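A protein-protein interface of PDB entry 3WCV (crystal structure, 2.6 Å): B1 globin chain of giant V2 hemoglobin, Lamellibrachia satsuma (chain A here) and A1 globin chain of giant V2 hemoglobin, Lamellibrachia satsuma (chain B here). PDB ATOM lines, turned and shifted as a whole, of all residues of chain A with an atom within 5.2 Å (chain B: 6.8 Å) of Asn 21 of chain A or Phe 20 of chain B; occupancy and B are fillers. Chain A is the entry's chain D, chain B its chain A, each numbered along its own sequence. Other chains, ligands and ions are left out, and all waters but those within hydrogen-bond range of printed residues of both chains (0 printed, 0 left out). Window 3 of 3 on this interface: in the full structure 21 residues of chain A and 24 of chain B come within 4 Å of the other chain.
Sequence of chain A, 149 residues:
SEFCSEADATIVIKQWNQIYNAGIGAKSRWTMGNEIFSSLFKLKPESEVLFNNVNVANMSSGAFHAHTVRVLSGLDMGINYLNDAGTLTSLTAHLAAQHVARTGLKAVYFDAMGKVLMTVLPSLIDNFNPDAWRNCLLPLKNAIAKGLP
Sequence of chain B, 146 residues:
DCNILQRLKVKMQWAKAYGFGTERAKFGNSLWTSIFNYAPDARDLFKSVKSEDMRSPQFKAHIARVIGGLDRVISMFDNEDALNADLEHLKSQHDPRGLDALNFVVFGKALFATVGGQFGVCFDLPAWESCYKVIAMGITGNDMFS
The guanidinium group (NH1) of Arg 24 of chain B sits close to the side-chain amide nitrogen (ND2) of Asn 80 of chain A, 3.1 Å away. OD2 of Asp 71 of chain B is in salt-bridge range of NH2 of Arg 29 of chain A, 3.2 Å away. The side-chain hydroxyl (OG) of Ser 75 of chain B sits at hydrogen-bond distance from the guanidinium group (NH2) of Arg 29 of chain A.
O of Gly 19 of chain B lies within hydrogen-bond range of NH2 of Arg 24 of chain B (3.3 Å). The side-chain amide nitrogen (ND2) of Asn 17 of chain A sits close to the backbone carbonyl oxygen (O) of Tyr 20 of chain A (3.1 Å). ND2 of Asn 21 of chain A sits at hydrogen-bond distance from O of Asn 17 of chain A (2.9 Å). The side-chain hydroxyl (OH) of Tyr 20 of chain A lies within hydrogen-bond range of the guanidinium group (NH2) of Arg 29 of chain A (3.0 Å). The side-chain amide oxygen (OD1) of Asn 21 of chain A is in hydrogen-bond range of the backbone NH (N) of Gly 23 of chain A, at 2.6 Å. O of Asn 21 of chain A lies within hydrogen-bond range of NH1 of Arg 29 of chain A, at 2.9 Å.
Among the printed residues, merely in contact across the chains: Tyr 20 of chain A with Asp 71 of chain B (3.97 Å), Asn 21 of chain A with Phe 20 of chain B (3.5 Å), Ala 22 of chain A with Ala 15 of chain B (3.4 Å), Ala 22 of chain A with Tyr 18 of chain B (3.9 Å), Ala 22 of chain A with Asp 71 of chain B (3.3 Å) and Asn 80 of chain A with Gly 21 of chain B (3.5 Å).
Printed residues of chain B within 4 Å of Tyr 20 of chain A: Asp 71 (3.97 Å). Of the printed residues of chain B, Asn 21 of chain A touches Phe 20 (3.5 Å). Ile 24 of chain A touches none of the printed residues of chain B. Printed residues of chain B within 4 Å of Arg 29 of chain A: Asp 71 (3.2 Å) and Ser 75 (3.2 Å). Of the printed residues of chain B, Asn 80 of chain A touches Gly 21 (3.5 Å) and Arg 24 (3.1 Å). Printed residues of chain A within 4 Å of Ala 15 of chain B: Ala 22. The nearest residue of chain B that does not touch Asn 21 of chain A is Asp 71 of chain B (5.4 Å).
Printed residues of chain A that touch a printed residue of chain B: Tyr 20, Asn 21, Ala 22, Arg 29 and Asn 80. Of the 12 printed residues of chain B, 7 touch a printed residue of chain A. Printed residues of chain B that touch a printed residue of chain A: Ala 15, Tyr 18, Phe 20, Gly 21, Arg 24, Asp 71 and Ser 75. Among the printed residues, 9 pairs touch across the chains. Among the printed residues, Asp or Glu carboxylates within 4 Å of a Lys or Arg side-chain nitrogen of the other chain: Arg 29 of chain A with Asp 71 of chain B (3.2 Å).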
ATOM      1  N   ASN A  17      36.151  12.164  13.223  1.00  0.00           N
ATOM      2  CA  ASN A  17      35.255  13.295  13.065  1.00  0.00           C
ATOM      3  C   ASN A  17      35.674  14.208  11.922  1.00  0.00           C
ATOM      4  O   ASN A  17      34.910  15.073  11.488  1.00  0.00           O
ATOM      5  CB  ASN A  17      35.138  14.049  14.387  1.00  0.00           C
ATOM      6  CG  ASN A  17      34.324  13.266  15.423  1.00  0.00           C
ATOM      7  OD1 ASN A  17      34.621  13.291  16.620  1.00  0.00           O
ATOM      8  ND2 ASN A  17      33.285  12.569  14.954  1.00  0.00           N
ATOM      9  N   GLN A  18      36.887  13.998  11.424  1.00  0.00           N
ATOM     10  CA  GLN A  18      37.413  14.762  10.295  1.00  0.00           C
ATOM     11  C   GLN A  18      36.577  14.452   9.073  1.00  0.00           C
ATOM     12  O   GLN A  18      36.180  15.339   8.325  1.00  0.00           O
ATOM     13  CB  GLN A  18      38.833  14.323   9.963  1.00  0.00           C
ATOM     14  CG  GLN A  18      39.943  15.228  10.384  1.00  0.00           C
ATOM     15  CD  GLN A  18      41.266  14.730   9.852  1.00  0.00           C
ATOM     16  OE1 GLN A  18      41.454  14.601   8.638  1.00  0.00           O
ATOM     17  NE2 GLN A  18      42.191  14.433  10.760  1.00  0.00           N
ATOM     18  N   ILE A  19      36.339  13.161   8.868  1.00  0.00           N
ATOM     19  CA  ILE A  19      35.584  12.687   7.717  1.00  0.00           C
ATOM     20  C   ILE A  19      34.134  12.304   8.003  1.00  0.00           C
ATOM     21  O   ILE A  19      33.396  11.981   7.078  1.00  0.00           O
ATOM     22  CB  ILE A  19      36.283  11.475   7.101  1.00  0.00           C
ATOM     23  CG1 ILE A  19      36.454  10.388   8.164  1.00  0.00           C
ATOM     24  CG2 ILE A  19      37.653  11.877   6.586  1.00  0.00           C
ATOM     25  CD1 ILE A  19      36.929   9.066   7.632  1.00  0.00           C
ATOM     26  N   TYR A  20      33.741  12.321   9.279  1.00  0.00           N
ATOM     27  CA  TYR A  20      32.369  11.962   9.658  1.00  0.00           C
ATOM     28  C   TYR A  20      31.864  12.718  10.842  1.00  0.00           C
ATOM     29  O   TYR A  20      32.507  12.697  11.931  1.00  0.00           O
ATOM     30  CB  TYR A  20      32.262  10.451   9.907  1.00  0.00           C
ATOM     31  CG  TYR A  20      30.855   9.947  10.181  1.00  0.00           C
ATOM     32  CD1 TYR A  20      30.200  10.237  11.377  1.00  0.00           C
ATOM     33  CD2 TYR A  20      30.178   9.181   9.238  1.00  0.00           C
ATOM     34  CE1 TYR A  20      28.894   9.773  11.625  1.00  0.00           C
ATOM     35  CE2 TYR A  20      28.877   8.713   9.475  1.00  0.00           C
ATOM     36  CZ  TYR A  20      28.241   9.011  10.667  1.00  0.00           C
ATOM     37  OH  TYR A  20      26.967   8.534  10.912  1.00  0.00           O
ATOM     38  N   ASN A  21      30.778  13.465  10.639  1.00  0.00           N
ATOM     39  CA  ASN A  21      30.164  14.185  11.730  1.00  0.00           C
ATOM     40  C   ASN A  21      28.802  14.648  11.257  1.00  0.00           C
ATOM     41  O   ASN A  21      28.538  14.627  10.053  1.00  0.00           O
ATOM     42  CB  ASN A  21      31.045  15.363  12.120  1.00  0.00           C
ATOM     43  CG  ASN A  21      31.267  16.310  10.964  1.00  0.00           C
ATOM     44  OD1 ASN A  21      30.299  16.954  10.483  1.00  0.00           O
ATOM     45  ND2 ASN A  21      32.530  16.386  10.474  1.00  0.00           N
ATOM     46  N   ALA A  22      27.949  15.065  12.190  1.00  0.00           N
ATOM     47  CA  ALA A  22      26.603  15.526  11.842  1.00  0.00           C
ATOM     48  C   ALA A  22      26.586  16.658  10.776  1.00  0.00           C
ATOM     49  O   ALA A  22      25.504  17.097  10.331  1.00  0.00           O
ATOM     50  CB  ALA A  22      25.876  16.007  13.128  1.00  0.00           C
ATOM     51  N   GLY A  23      27.755  17.210  10.442  1.00  0.00           N
ATOM     52  CA  GLY A  23      27.791  18.286   9.454  1.00  0.00           C
ATOM     53  C   GLY A  23      27.844  18.061   7.940  1.00  0.00           C
ATOM     54  O   GLY A  23      27.559  19.032   7.186  1.00  0.00           O
ATOM     55  N   ILE A  24      28.242  16.877   7.467  1.00  0.00           N
ATOM     56  CA  ILE A  24      28.194  16.730   6.040  1.00  0.00           C
ATOM     57  C   ILE A  24      27.376  15.611   5.415  1.00  0.00           C
ATOM     58  O   ILE A  24      27.097  14.504   5.995  1.00  0.00           O
ATOM     59  CB  ILE A  24      29.631  16.726   5.421  1.00  0.00           C
ATOM     60  CG1 ILE A  24      30.666  16.283   6.487  1.00  0.00           C
ATOM     61  CG2 ILE A  24      29.876  18.150   4.851  1.00  0.00           C
ATOM     62  CD1 ILE A  24      30.686  14.773   6.676  1.00  0.00           C
ATOM     63  N   ARG A  29      28.665  10.008   2.991  1.00  0.00           N
ATOM     64  CA  ARG A  29      28.527   8.884   3.914  1.00  0.00           C
ATOM     65  C   ARG A  29      28.459   7.552   3.198  1.00  0.00           C
ATOM     66  O   ARG A  29      29.174   6.622   3.556  1.00  0.00           O
ATOM     67  CB  ARG A  29      27.289   9.064   4.791  1.00  0.00           C
ATOM     68  CG  ARG A  29      27.620   9.664   6.135  1.00  0.00           C
ATOM     69  CD  ARG A  29      26.393  10.120   6.901  1.00  0.00           C
ATOM     70  NE  ARG A  29      26.743  11.238   7.779  1.00  0.00           N
ATOM     71  CZ  ARG A  29      26.209  11.447   8.975  1.00  0.00           C
ATOM     72  NH1 ARG A  29      26.595  12.492   9.689  1.00  0.00           N
ATOM     73  NH2 ARG A  29      25.302  10.607   9.466  1.00  0.00           N
ATOM     74  N   ASN A  80      32.705   7.230  19.281  1.00  0.00           N
ATOM     75  CA  ASN A  80      32.347   8.290  20.215  1.00  0.00           C
ATOM     76  C   ASN A  80      32.125   7.793  21.647  1.00  0.00           C
ATOM     77  O   ASN A  80      31.952   8.585  22.579  1.00  0.00           O
ATOM     78  CB  ASN A  80      31.105   9.019  19.713  1.00  0.00           C
ATOM     79  CG  ASN A  80      31.420   9.968  18.586  1.00  0.00           C
ATOM     80  OD1 ASN A  80      31.681  11.146  18.803  1.00  0.00           O
ATOM     81  ND2 ASN A  80      31.419   9.454  17.370  1.00  0.00           N
ATOM     82  N   ALA B  15      23.128  19.531  13.815  1.00  0.00           N
ATOM     83  CA  ALA B  15      24.570  19.336  13.929  1.00  0.00           C
ATOM     84  C   ALA B  15      25.144  20.177  15.062  1.00  0.00           C
ATOM     85  O   ALA B  15      25.958  19.699  15.832  1.00  0.00           O
ATOM     86  CB  ALA B  15      25.265  19.662  12.607  1.00  0.00           C
ATOM     87  N   LYS B  16      24.709  21.423  15.163  1.00  0.00           N
ATOM     88  CA  LYS B  16      25.168  22.302  16.224  1.00  0.00           C
ATOM     89  C   LYS B  16      24.724  21.711  17.582  1.00  0.00           C
ATOM     90  O   LYS B  16      25.547  21.349  18.400  1.00  0.00           O
ATOM     91  CB  LYS B  16      24.583  23.709  16.002  1.00  0.00           C
ATOM     92  CG  LYS B  16      25.024  24.769  17.004  1.00  0.00           C
ATOM     93  CD  LYS B  16      26.546  24.963  16.987  1.00  0.00           C
ATOM     94  CE  LYS B  16      26.985  26.052  17.955  1.00  0.00           C
ATOM     95  NZ  LYS B  16      28.467  26.201  18.009  1.00  0.00           N
ATOM     96  N   TYR B  18      23.566  18.839  18.545  1.00  0.00           N
ATOM     97  CA  TYR B  18      24.018  17.473  18.803  1.00  0.00           C
ATOM     98  C   TYR B  18      25.481  17.416  19.255  1.00  0.00           C
ATOM     99  O   TYR B  18      25.834  16.639  20.138  1.00  0.00           O
ATOM    100  CB  TYR B  18      23.819  16.665  17.530  1.00  0.00           C
ATOM    101  CG  TYR B  18      24.202  15.219  17.604  1.00  0.00           C
ATOM    102  CD1 TYR B  18      23.619  14.380  18.549  1.00  0.00           C
ATOM    103  CD2 TYR B  18      25.066  14.655  16.651  1.00  0.00           C
ATOM    104  CE1 TYR B  18      23.869  13.015  18.550  1.00  0.00           C
ATOM    105  CE2 TYR B  18      25.327  13.286  16.641  1.00  0.00           C
ATOM    106  CZ  TYR B  18      24.716  12.472  17.595  1.00  0.00           C
ATOM    107  OH  TYR B  18      24.931  11.108  17.574  1.00  0.00           O
ATOM    108  N   GLY B  19      26.317  18.234  18.627  1.00  0.00           N
ATOM    109  CA  GLY B  19      27.721  18.295  18.981  1.00  0.00           C
ATOM    110  C   GLY B  19      28.554  17.045  18.799  1.00  0.00           C
ATOM    111  O   GLY B  19      28.111  16.025  18.264  1.00  0.00           O
ATOM    112  N   PHE B  20      29.788  17.144  19.268  1.00  0.00           N
ATOM    113  CA  PHE B  20      30.741  16.055  19.187  1.00  0.00           C
ATOM    114  C   PHE B  20      30.953  15.355  20.541  1.00  0.00           C
ATOM    115  O   PHE B  20      30.463  15.799  21.587  1.00  0.00           O
ATOM    116  CB  PHE B  20      32.074  16.606  18.677  1.00  0.00           C
ATOM    117  CG  PHE B  20      31.979  17.280  17.341  1.00  0.00           C
ATOM    118  CD1 PHE B  20      32.020  16.534  16.172  1.00  0.00           C
ATOM    119  CD2 PHE B  20      31.882  18.667  17.247  1.00  0.00           C
ATOM    120  CE1 PHE B  20      31.970  17.165  14.919  1.00  0.00           C
ATOM    121  CE2 PHE B  20      31.831  19.309  16.000  1.00  0.00           C
ATOM    122  CZ  PHE B  20      31.877  18.557  14.834  1.00  0.00           C
ATOM    123  N   GLY B  21      31.682  14.247  20.485  1.00  0.00           N
ATOM    124  CA  GLY B  21      32.022  13.470  21.666  1.00  0.00           C
ATOM    125  C   GLY B  21      31.027  13.309  22.790  1.00  0.00           C
ATOM    126  O   GLY B  21      29.861  13.025  22.565  1.00  0.00           O
ATOM    127  N   THR B  22      31.513  13.490  24.012  1.00  0.00           N
ATOM    128  CA  THR B  22      30.715  13.342  25.225  1.00  0.00           C
ATOM    129  C   THR B  22      29.515  14.280  25.346  1.00  0.00           C
ATOM    130  O   THR B  22      28.589  13.995  26.094  1.00  0.00           O
ATOM    131  CB  THR B  22      31.605  13.538  26.472  1.00  0.00           C
ATOM    132  OG1 THR B  22      32.033  14.908  26.550  1.00  0.00           O
ATOM    133  CG2 THR B  22      32.847  12.647  26.376  1.00  0.00           C
ATOM    134  N   GLU B  23      29.528  15.402  24.631  1.00  0.00           N
ATOM    135  CA  GLU B  23      28.415  16.345  24.699  1.00  0.00           C
ATOM    136  C   GLU B  23      27.162  15.699  24.121  1.00  0.00           C
ATOM    137  O   GLU B  23      26.029  16.089  24.421  1.00  0.00           O
ATOM    138  CB  GLU B  23      28.753  17.629  23.931  1.00  0.00           C
ATOM    139  CG  GLU B  23      29.681  18.571  24.680  1.00  0.00           C
ATOM    140  CD  GLU B  23      29.275  18.748  26.147  1.00  0.00           C
ATOM    141  OE1 GLU B  23      29.509  17.806  26.944  1.00  0.00           O
ATOM    142  OE2 GLU B  23      28.718  19.816  26.504  1.00  0.00           O
ATOM    143  N   ARG B  24      27.405  14.694  23.294  1.00  0.00           N
ATOM    144  CA  ARG B  24      26.380  13.919  22.637  1.00  0.00           C
ATOM    145  C   ARG B  24      25.560  13.140  23.682  1.00  0.00           C
ATOM    146  O   ARG B  24      24.325  13.166  23.659  1.00  0.00           O
ATOM    147  CB  ARG B  24      27.080  12.984  21.658  1.00  0.00           C
ATOM    148  CG  ARG B  24      26.208  12.201  20.745  1.00  0.00           C
ATOM    149  CD  ARG B  24      27.094  11.525  19.716  1.00  0.00           C
ATOM    150  NE  ARG B  24      27.784  12.487  18.858  1.00  0.00           N
ATOM    151  CZ  ARG B  24      28.532  12.143  17.806  1.00  0.00           C
ATOM    152  NH1 ARG B  24      28.682  10.860  17.492  1.00  0.00           N
ATOM    153  NH2 ARG B  24      29.128  13.079  17.072  1.00  0.00           N
ATOM    154  N   ALA B  25      26.241  12.464  24.604  1.00  0.00           N
ATOM    155  CA  ALA B  25      25.544  11.703  25.630  1.00  0.00           C
ATOM    156  C   ALA B  25      24.669  12.633  26.482  1.00  0.00           C
ATOM    157  O   ALA B  25      23.538  12.301  26.809  1.00  0.00           O
ATOM    158  CB  ALA B  25      26.554  10.952  26.501  1.00  0.00           C
ATOM    159  N   ASP B  71      20.276  11.042  14.091  1.00  0.00           N
ATOM    160  CA  ASP B  71      21.368  11.604  13.295  1.00  0.00           C
ATOM    161  C   ASP B  71      21.518  11.055  11.875  1.00  0.00           C
ATOM    162  O   ASP B  71      21.673  11.824  10.922  1.00  0.00           O
ATOM    163  CB  ASP B  71      22.710  11.458  14.011  1.00  0.00           C
ATOM    164  CG  ASP B  71      23.863  12.052  13.199  1.00  0.00           C
ATOM    165  OD1 ASP B  71      24.017  13.303  13.242  1.00  0.00           O
ATOM    166  OD2 ASP B  71      24.587  11.278  12.503  1.00  0.00           O
ATOM    167  N   SER B  75      20.647  13.039   8.420  1.00  0.00           N
ATOM    168  CA  SER B  75      21.693  13.194   7.407  1.00  0.00           C
ATOM    169  C   SER B  75      21.223  12.771   6.032  1.00  0.00           C
ATOM    170  O   SER B  75      21.778  13.212   5.040  1.00  0.00           O
ATOM    171  CB  SER B  75      22.956  12.392   7.761  1.00  0.00           C
ATOM    172  OG  SER B  75      22.809  11.010   7.468  1.00  0.00           O
